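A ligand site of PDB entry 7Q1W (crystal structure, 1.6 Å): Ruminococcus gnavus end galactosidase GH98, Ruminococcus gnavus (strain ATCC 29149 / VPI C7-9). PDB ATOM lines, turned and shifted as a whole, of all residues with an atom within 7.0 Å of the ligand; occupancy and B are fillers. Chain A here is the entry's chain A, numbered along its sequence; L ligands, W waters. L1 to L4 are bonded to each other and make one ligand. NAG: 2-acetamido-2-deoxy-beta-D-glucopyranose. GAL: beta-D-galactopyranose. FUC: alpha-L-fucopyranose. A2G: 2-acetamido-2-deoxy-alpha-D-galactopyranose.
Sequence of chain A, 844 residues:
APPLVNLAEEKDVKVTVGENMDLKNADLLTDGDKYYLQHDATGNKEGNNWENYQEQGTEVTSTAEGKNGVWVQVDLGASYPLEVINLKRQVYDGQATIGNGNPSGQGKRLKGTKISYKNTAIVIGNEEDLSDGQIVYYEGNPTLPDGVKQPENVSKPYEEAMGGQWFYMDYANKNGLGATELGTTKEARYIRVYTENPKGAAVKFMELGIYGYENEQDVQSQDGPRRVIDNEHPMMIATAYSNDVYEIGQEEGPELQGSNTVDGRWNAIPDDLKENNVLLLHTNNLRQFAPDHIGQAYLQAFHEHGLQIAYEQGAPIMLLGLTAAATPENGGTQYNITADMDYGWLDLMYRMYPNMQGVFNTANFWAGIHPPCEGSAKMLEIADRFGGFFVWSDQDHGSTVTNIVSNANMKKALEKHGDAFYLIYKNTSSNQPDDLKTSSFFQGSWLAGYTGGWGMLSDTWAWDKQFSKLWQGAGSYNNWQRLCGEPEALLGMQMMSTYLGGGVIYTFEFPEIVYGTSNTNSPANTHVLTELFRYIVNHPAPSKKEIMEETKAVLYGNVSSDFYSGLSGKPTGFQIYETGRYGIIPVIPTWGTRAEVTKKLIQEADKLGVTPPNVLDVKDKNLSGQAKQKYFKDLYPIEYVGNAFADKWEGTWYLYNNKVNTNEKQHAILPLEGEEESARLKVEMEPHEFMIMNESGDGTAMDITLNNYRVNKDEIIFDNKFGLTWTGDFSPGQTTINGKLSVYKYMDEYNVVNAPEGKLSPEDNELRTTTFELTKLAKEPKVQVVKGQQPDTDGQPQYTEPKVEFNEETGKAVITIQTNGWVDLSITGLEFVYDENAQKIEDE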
ATOM      1  N   LEU A 470       3.302  11.363  12.872  1.00  0.00           N
ATOM      2  CA  LEU A 470       4.460  11.962  12.185  1.00  0.00           C
ATOM      3  C   LEU A 470       5.087  10.935  11.234  1.00  0.00           C
ATOM      4  O   LEU A 470       5.341   9.789  11.640  1.00  0.00           O
ATOM      5  CB  LEU A 470       5.453  12.409  13.252  1.00  0.00           C
ATOM      6  CG  LEU A 470       6.662  13.190  12.744  1.00  0.00           C
ATOM      7  CD1 LEU A 470       6.267  14.481  12.066  1.00  0.00           C
ATOM      8  CD2 LEU A 470       7.605  13.476  13.886  1.00  0.00           C
ATOM      9  N   TRP A 471       5.274  11.339   9.980  1.00  0.00           N
ATOM     10  CA  TRP A 471       5.928  10.530   8.906  1.00  0.00           C
ATOM     11  C   TRP A 471       4.985   9.447   8.351  1.00  0.00           C
ATOM     12  O   TRP A 471       5.448   8.668   7.494  1.00  0.00           O
ATOM     13  CB  TRP A 471       7.231   9.869   9.405  1.00  0.00           C
ATOM     14  CG  TRP A 471       8.150  10.767  10.190  1.00  0.00           C
ATOM     15  CD1 TRP A 471       8.746  10.426  11.355  1.00  0.00           C
ATOM     16  CD2 TRP A 471       8.554  12.127   9.900  1.00  0.00           C
ATOM     17  NE1 TRP A 471       9.537  11.462  11.794  1.00  0.00           N
ATOM     18  CE2 TRP A 471       9.476  12.494  10.906  1.00  0.00           C
ATOM     19  CE3 TRP A 471       8.307  13.019   8.846  1.00  0.00           C
ATOM     20  CZ2 TRP A 471      10.065  13.770  10.958  1.00  0.00           C
ATOM     21  CZ3 TRP A 471       8.956  14.239   8.857  1.00  0.00           C
ATOM     22  CH2 TRP A 471       9.795  14.621   9.908  1.00  0.00           C
ATOM     23  N   ASN A 663      10.765  12.416   6.394  1.00  0.00           N
ATOM     24  CA  ASN A 663      11.854  12.903   7.266  1.00  0.00           C
ATOM     25  C   ASN A 663      13.146  12.959   6.439  1.00  0.00           C
ATOM     26  O   ASN A 663      13.945  12.013   6.509  1.00  0.00           O
ATOM     27  CB  ASN A 663      12.021  12.020   8.492  1.00  0.00           C
ATOM     28  CG  ASN A 663      13.018  12.611   9.471  1.00  0.00           C
ATOM     29  OD1 ASN A 663      13.426  13.761   9.343  1.00  0.00           O
ATOM     30  ND2 ASN A 663      13.384  11.833  10.465  1.00  0.00           N
ATOM     31  N   LYS A 665      16.497  15.720   5.300  1.00  0.00           N
ATOM     32  CA  LYS A 665      17.203  17.013   5.398  1.00  0.00           C
ATOM     33  C   LYS A 665      17.202  17.679   4.025  1.00  0.00           C
ATOM     34  O   LYS A 665      17.224  16.966   3.014  1.00  0.00           O
ATOM     35  CB  LYS A 665      18.665  16.826   5.853  1.00  0.00           C
ATOM     36  CG  LYS A 665      18.840  16.139   7.193  1.00  0.00           C
ATOM     37  CD  LYS A 665      20.308  15.879   7.548  1.00  0.00           C
ATOM     38  CE  LYS A 665      20.493  15.273   8.929  1.00  0.00           C
ATOM     39  NZ  LYS A 665      20.118  16.257   9.991  1.00  0.00           N
ATOM     40  N   GLU A 686      16.107  20.009   8.872  1.00  0.00           N
ATOM     41  CA  GLU A 686      15.159  18.878   8.889  1.00  0.00           C
ATOM     42  C   GLU A 686      13.764  19.461   8.703  1.00  0.00           C
ATOM     43  O   GLU A 686      13.598  20.678   8.732  1.00  0.00           O
ATOM     44  CB  GLU A 686      15.306  18.127  10.212  1.00  0.00           C
ATOM     45  CG  GLU A 686      16.725  17.581  10.373  1.00  0.00           C
ATOM     46  CD  GLU A 686      16.943  16.649  11.547  1.00  0.00           C
ATOM     47  OE1 GLU A 686      15.922  16.224  12.178  1.00  0.00           O
ATOM     48  OE2 GLU A 686      18.133  16.352  11.845  1.00  0.00           O
ATOM     49  N   ARG A 710       7.297  22.067  16.883  1.00  0.00           N
ATOM     50  CA  ARG A 710       6.467  20.882  16.567  1.00  0.00           C
ATOM     51  C   ARG A 710       6.157  20.124  17.847  1.00  0.00           C
ATOM     52  O   ARG A 710       7.086  19.694  18.571  1.00  0.00           O
ATOM     53  CB  ARG A 710       7.095  19.984  15.511  1.00  0.00           C
ATOM     54  CG  ARG A 710       6.149  18.875  15.054  1.00  0.00           C
ATOM     55  CD  ARG A 710       6.809  18.020  14.008  1.00  0.00           C
ATOM     56  NE  ARG A 710       7.892  17.221  14.583  1.00  0.00           N
ATOM     57  CZ  ARG A 710       9.041  16.891  13.983  1.00  0.00           C
ATOM     58  NH1 ARG A 710       9.241  17.190  12.705  1.00  0.00           N
ATOM     59  NH2 ARG A 710       9.948  16.190  14.651  1.00  0.00           N
ATOM     60  N   ASN A 765       9.600  18.742  23.364  1.00  0.00           N
ATOM     61  CA  ASN A 765      10.955  18.762  23.983  1.00  0.00           C
ATOM     62  C   ASN A 765      11.966  17.976  23.146  1.00  0.00           C
ATOM     63  O   ASN A 765      13.185  18.013  23.503  1.00  0.00           O
ATOM     64  CB  ASN A 765      10.880  18.240  25.406  1.00  0.00           C
ATOM     65  CG  ASN A 765      10.012  19.160  26.227  1.00  0.00           C
ATOM     66  OD1 ASN A 765      10.064  20.359  26.017  1.00  0.00           O
ATOM     67  ND2 ASN A 765       9.211  18.614  27.130  1.00  0.00           N
ATOM     68  N   GLU A 766      11.537  17.247  22.111  1.00  0.00           N
ATOM     69  CA  GLU A 766      12.495  16.490  21.265  1.00  0.00           C
ATOM     70  C   GLU A 766      13.103  17.470  20.261  1.00  0.00           C
ATOM     71  O   GLU A 766      12.351  18.026  19.438  1.00  0.00           O
ATOM     72  CB  GLU A 766      11.854  15.303  20.550  1.00  0.00           C
ATOM     73  CG  GLU A 766      12.902  14.417  19.855  1.00  0.00           C
ATOM     74  CD  GLU A 766      12.410  13.276  18.954  1.00  0.00           C
ATOM     75  OE1 GLU A 766      11.255  12.868  19.098  1.00  0.00           O
ATOM     76  OE2 GLU A 766      13.209  12.769  18.139  1.00  0.00           O
ATOM     77  N   LEU A 767      14.419  17.678  20.318  1.00  0.00           N
ATOM     78  CA  LEU A 767      15.060  18.744  19.521  1.00  0.00           C
ATOM     79  C   LEU A 767      15.585  18.195  18.187  1.00  0.00           C
ATOM     80  O   LEU A 767      15.925  16.989  18.071  1.00  0.00           O
ATOM     81  CB  LEU A 767      16.179  19.398  20.317  1.00  0.00           C
ATOM     82  CG  LEU A 767      15.848  19.803  21.749  1.00  0.00           C
ATOM     83  CD1 LEU A 767      17.091  20.454  22.359  1.00  0.00           C
ATOM     84  CD2 LEU A 767      14.633  20.736  21.790  1.00  0.00           C
ATOM     85  N   ARG A 768      15.652  19.071  17.188  1.00  0.00           N
ATOM     86  CA  ARG A 768      16.202  18.687  15.863  1.00  0.00           C
ATOM     87  C   ARG A 768      17.312  19.649  15.468  1.00  0.00           C
ATOM     88  O   ARG A 768      17.254  20.833  15.815  1.00  0.00           O
ATOM     89  CB  ARG A 768      15.106  18.715  14.787  1.00  0.00           C
ATOM     90  CG  ARG A 768      14.064  17.618  14.974  1.00  0.00           C
ATOM     91  CD  ARG A 768      12.731  18.086  15.486  1.00  0.00           C
ATOM     92  NE  ARG A 768      12.069  18.841  14.436  1.00  0.00           N
ATOM     93  CZ  ARG A 768      11.196  19.796  14.615  1.00  0.00           C
ATOM     94  NH1 ARG A 768      10.851  20.146  15.832  1.00  0.00           N
ATOM     95  NH2 ARG A 768      10.727  20.463  13.575  1.00  0.00           N
ATOM     96  N   THR A 769      18.234  19.140  14.662  1.00  0.00           N
ATOM     97  CA  THR A 769      19.497  19.816  14.329  1.00  0.00           C
ATOM     98  C   THR A 769      19.335  20.717  13.110  1.00  0.00           C
ATOM     99  O   THR A 769      18.796  20.265  12.092  1.00  0.00           O
ATOM    100  CB  THR A 769      20.599  18.775  14.103  1.00  0.00           C
ATOM    101  OG1 THR A 769      20.787  18.118  15.359  1.00  0.00           O
ATOM    102  CG2 THR A 769      21.883  19.430  13.670  1.00  0.00           C
ATOM    103  N   THR A 770      19.827  21.957  13.231  1.00  0.00           N
ATOM    104  CA  THR A 770      20.118  22.856  12.083  1.00  0.00           C
ATOM    105  C   THR A 770      21.630  23.070  12.024  1.00  0.00           C
ATOM    106  O   THR A 770      22.256  23.291  13.092  1.00  0.00           O
ATOM    107  CB  THR A 770      19.344  24.181  12.184  1.00  0.00           C
ATOM    108  OG1 THR A 770      17.947  23.917  12.351  1.00  0.00           O
ATOM    109  CG2 THR A 770      19.544  24.998  10.939  1.00  0.00           C
ATOM    110  N   THR A 771      22.198  23.031  10.824  1.00  0.00           N
ATOM    111  CA  THR A 771      23.641  23.310  10.647  1.00  0.00           C
ATOM    112  C   THR A 771      23.805  24.446   9.627  1.00  0.00           C
ATOM    113  O   THR A 771      23.019  24.561   8.653  1.00  0.00           O
ATOM    114  CB  THR A 771      24.399  22.004  10.369  1.00  0.00           C
ATOM    115  OG1 THR A 771      24.241  21.787   8.979  1.00  0.00           O
ATOM    116  CG2 THR A 771      23.864  20.832  11.166  1.00  0.00           C
ATOM    117  N   THR A 800      19.476  24.074  22.541  1.00  0.00           N
ATOM    118  CA  THR A 800      20.842  23.897  23.091  1.00  0.00           C
ATOM    119  C   THR A 800      21.710  25.056  22.610  1.00  0.00           C
ATOM    120  O   THR A 800      21.367  25.701  21.626  1.00  0.00           O
ATOM    121  CB  THR A 800      21.448  22.570  22.631  1.00  0.00           C
ATOM    122  OG1 THR A 800      21.439  22.540  21.203  1.00  0.00           O
ATOM    123  CG2 THR A 800      20.710  21.371  23.183  1.00  0.00           C
ATOM    124  N   THR A 816      26.404  24.348  14.639  1.00  0.00           N
ATOM    125  CA  THR A 816      25.353  23.338  14.866  1.00  0.00           C
ATOM    126  C   THR A 816      24.448  23.824  15.999  1.00  0.00           C
ATOM    127  O   THR A 816      24.955  24.239  17.020  1.00  0.00           O
ATOM    128  CB  THR A 816      26.025  21.979  15.113  1.00  0.00           C
ATOM    129  OG1 THR A 816      26.842  21.729  13.974  1.00  0.00           O
ATOM    130  CG2 THR A 816      25.021  20.864  15.266  1.00  0.00           C
ATOM    131  N   ILE A 817      23.140  23.703  15.856  1.00  0.00           N
ATOM    132  CA  ILE A 817      22.210  23.989  16.979  1.00  0.00           C
ATOM    133  C   ILE A 817      21.068  22.968  16.930  1.00  0.00           C
ATOM    134  O   ILE A 817      20.763  22.444  15.827  1.00  0.00           O
ATOM    135  CB  ILE A 817      21.710  25.444  16.933  1.00  0.00           C
ATOM    136  CG1 ILE A 817      21.069  25.803  18.268  1.00  0.00           C
ATOM    137  CG2 ILE A 817      20.778  25.660  15.746  1.00  0.00           C
ATOM    138  CD1 ILE A 817      20.676  27.264  18.390  1.00  0.00           C
ATOM    139  N   GLN A 818      20.525  22.650  18.093  1.00  0.00           N
ATOM    140  CA  GLN A 818      19.353  21.747  18.241  1.00  0.00           C
ATOM    141  C   GLN A 818      18.211  22.602  18.793  1.00  0.00           C
ATOM    142  O   GLN A 818      18.397  23.346  19.783  1.00  0.00           O
ATOM    143  CB  GLN A 818      19.642  20.573  19.169  1.00  0.00           C
ATOM    144  CG  GLN A 818      20.767  19.673  18.685  1.00  0.00           C
ATOM    145  CD  GLN A 818      20.425  18.266  19.109  1.00  0.00           C
ATOM    146  OE1 GLN A 818      19.957  17.446  18.304  1.00  0.00           O
ATOM    147  NE2 GLN A 818      20.492  18.032  20.409  1.00  0.00           N
HETATM  148  C1  NAG L   1      20.740   9.950  24.943  1.00  0.00           C
HETATM  149  C2  NAG L   1      21.934   9.679  24.028  1.00  0.00           C
HETATM  150  C3  NAG L   1      21.900  10.635  22.838  1.00  0.00           C
HETATM  151  C4  NAG L   1      20.538  10.541  22.159  1.00  0.00           C
HETATM  152  C5  NAG L   1      19.429  10.840  23.173  1.00  0.00           C
HETATM  153  C6  NAG L   1      18.038  10.736  22.594  1.00  0.00           C
HETATM  154  C7  NAG L   1      24.083   8.745  24.767  1.00  0.00           C
HETATM  155  C8  NAG L   1      25.114   8.818  25.858  1.00  0.00           C
HETATM  156  N2  NAG L   1      23.221   9.761  24.701  1.00  0.00           N
HETATM  157  O1  NAG L   1      20.725   9.006  25.968  1.00  0.00           O
HETATM  158  O3  NAG L   1      22.932  10.307  21.920  1.00  0.00           O
HETATM  159  O4  NAG L   1      20.488  11.505  21.099  1.00  0.00           O
HETATM  160  O5  NAG L   1      19.510   9.876  24.239  1.00  0.00           O
HETATM  161  O6  NAG L   1      17.799   9.452  22.025  1.00  0.00           O
HETATM  162  O7  NAG L   1      24.052   7.817  23.972  1.00  0.00           O
HETATM  163  C1  GAL L   2      20.120  11.053  19.829  1.00  0.00           C
HETATM  164  C2  GAL L   2      19.800  12.276  18.967  1.00  0.00           C
HETATM  165  C3  GAL L   2      19.460  11.819  17.550  1.00  0.00           C
HETATM  166  C4  GAL L   2      20.581  10.957  16.971  1.00  0.00           C
HETATM  167  C5  GAL L   2      20.920   9.818  17.919  1.00  0.00           C
HETATM  168  C6  GAL L   2      22.139   9.034  17.470  1.00  0.00           C
HETATM  169  O2  GAL L   2      18.706  13.012  19.537  1.00  0.00           O
HETATM  170  O3  GAL L   2      19.307  12.977  16.713  1.00  0.00           O
HETATM  171  O4  GAL L   2      21.738  11.759  16.753  1.00  0.00           O
HETATM  172  O5  GAL L   2      21.194  10.317  19.245  1.00  0.00           O
HETATM  173  O6  GAL L   2      22.444   7.985  18.380  1.00  0.00           O
HETATM  174  C1  FUC L   3      18.868  14.420  19.536  1.00  0.00           C
HETATM  175  C2  FUC L   3      17.566  15.118  19.921  1.00  0.00           C
HETATM  176  C3  FUC L   3      17.259  15.042  21.433  1.00  0.00           C
HETATM  177  C4  FUC L   3      18.500  15.397  22.260  1.00  0.00           C
HETATM  178  C5  FUC L   3      19.692  14.555  21.807  1.00  0.00           C
HETATM  179  C6  FUC L   3      20.972  14.884  22.534  1.00  0.00           C
HETATM  180  O2  FUC L   3      16.504  14.562  19.147  1.00  0.00           O
HETATM  181  O3  FUC L   3      16.176  15.917  21.786  1.00  0.00           O
HETATM  182  O4  FUC L   3      18.809  16.786  22.125  1.00  0.00           O
HETATM  183  O5  FUC L   3      19.938  14.805  20.400  1.00  0.00           O
HETATM  184  O5  A2G L   4      17.416  12.377  15.481  1.00  0.00           O
HETATM  185  C1  A2G L   4      18.791  12.771  15.421  1.00  0.00           C
HETATM  186  C2  A2G L   4      19.010  14.035  14.627  1.00  0.00           C
HETATM  187  N2  A2G L   4      20.409  14.444  14.597  1.00  0.00           N
HETATM  188  C3  A2G L   4      18.095  15.137  15.162  1.00  0.00           C
HETATM  189  O3  A2G L   4      18.245  16.303  14.355  1.00  0.00           O
HETATM  190  C4  A2G L   4      16.647  14.660  15.171  1.00  0.00           C
HETATM  191  O4  A2G L   4      16.203  14.370  13.850  1.00  0.00           O
HETATM  192  C5  A2G L   4      16.529  13.389  16.000  1.00  0.00           C
HETATM  193  C6  A2G L   4      15.135  12.804  15.968  1.00  0.00           C
HETATM  194  O6  A2G L   4      14.132  13.833  16.045  1.00  0.00           O
HETATM  195  C7  A2G L   4      21.109  14.742  13.494  1.00  0.00           C
HETATM  196  O7  A2G L   4      20.605  14.756  12.368  1.00  0.00           O
HETATM  197  C8  A2G L   4      22.551  15.092  13.697  1.00  0.00           C
HETATM  198  O   HOH W   1      12.281  14.602  13.847  1.00  0.00           O
HETATM  199  O   HOH W   2      15.645  12.301  19.443  1.00  0.00           O
HETATM  200  O   HOH W   3      24.348  17.378  15.318  1.00  0.00           O
HETATM  201  O   HOH W   4      22.098  14.400  17.059  1.00  0.00           O
HETATM  202  O   HOH W   5      13.417  10.161  14.469  1.00  0.00           O
HETATM  203  O   HOH W   6      15.436  12.307  12.439  1.00  0.00           O
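The side-chain carboxylate of Glu 686 sits at hydrogen-bond distance from an oxygen (O4) of A2G L4 (2.5 Å). The side-chain carboxylate (OE2) of Glu 766 sits at hydrogen-bond distance from an oxygen (O6) of A2G L4 (2.5 Å). NE2 of Gln 818 lies within hydrogen-bond range of O4 of FUC L3, at 2.7 Å. O3 of FUC L3 sits at hydrogen-bond distance from N of Leu 767 (2.9 Å). An oxygen (O2) of FUC L3 lies within hydrogen-bond range of the backbone carbonyl oxygen of Leu 767 (2.7 Å). NZ of Lys 665 sits at hydrogen-bond distance from O7 of A2G L4 (2.9 Å). N of Thr 769 is in hydrogen-bond range of O3 of A2G L4. OG1 of Thr 769 lies within hydrogen-bond range of O3 of A2G L4 (3.3 Å).
Water W2 lies within hydrogen-bond range of O2 of FUC L3 (2.4 Å) and OE2 of Glu 766 (2.8 Å). Water W6 lies within hydrogen-bond range of O4 of A2G L4 (2.6 Å) and ND2 of Asn 663 (2.9 Å). Water W1 lies within hydrogen-bond range of the guanidinium group (NH2) of Arg 710 (2.9 Å) and an oxygen (O6) of A2G L4 (3.0 Å).
Arg 768 touches the ligand. Hydrophobic or aromatic side chains within 4 Å of the ligand: Leu 767. Of the 17 residues printed, 7 come within 4 Å of the ligand.
NZ of Lys 665 lies within salt-bridge range of OE2 of Glu 686, 2.7 Å away. The side-chain amide oxygen of Gln 818 is in hydrogen-bond range of the side-chain hydroxyl of Thr 769 (3.1 Å). The backbone NH of Thr 800 lies within hydrogen-bond range of the backbone carbonyl oxygen of Gln 818 (3.0 Å).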
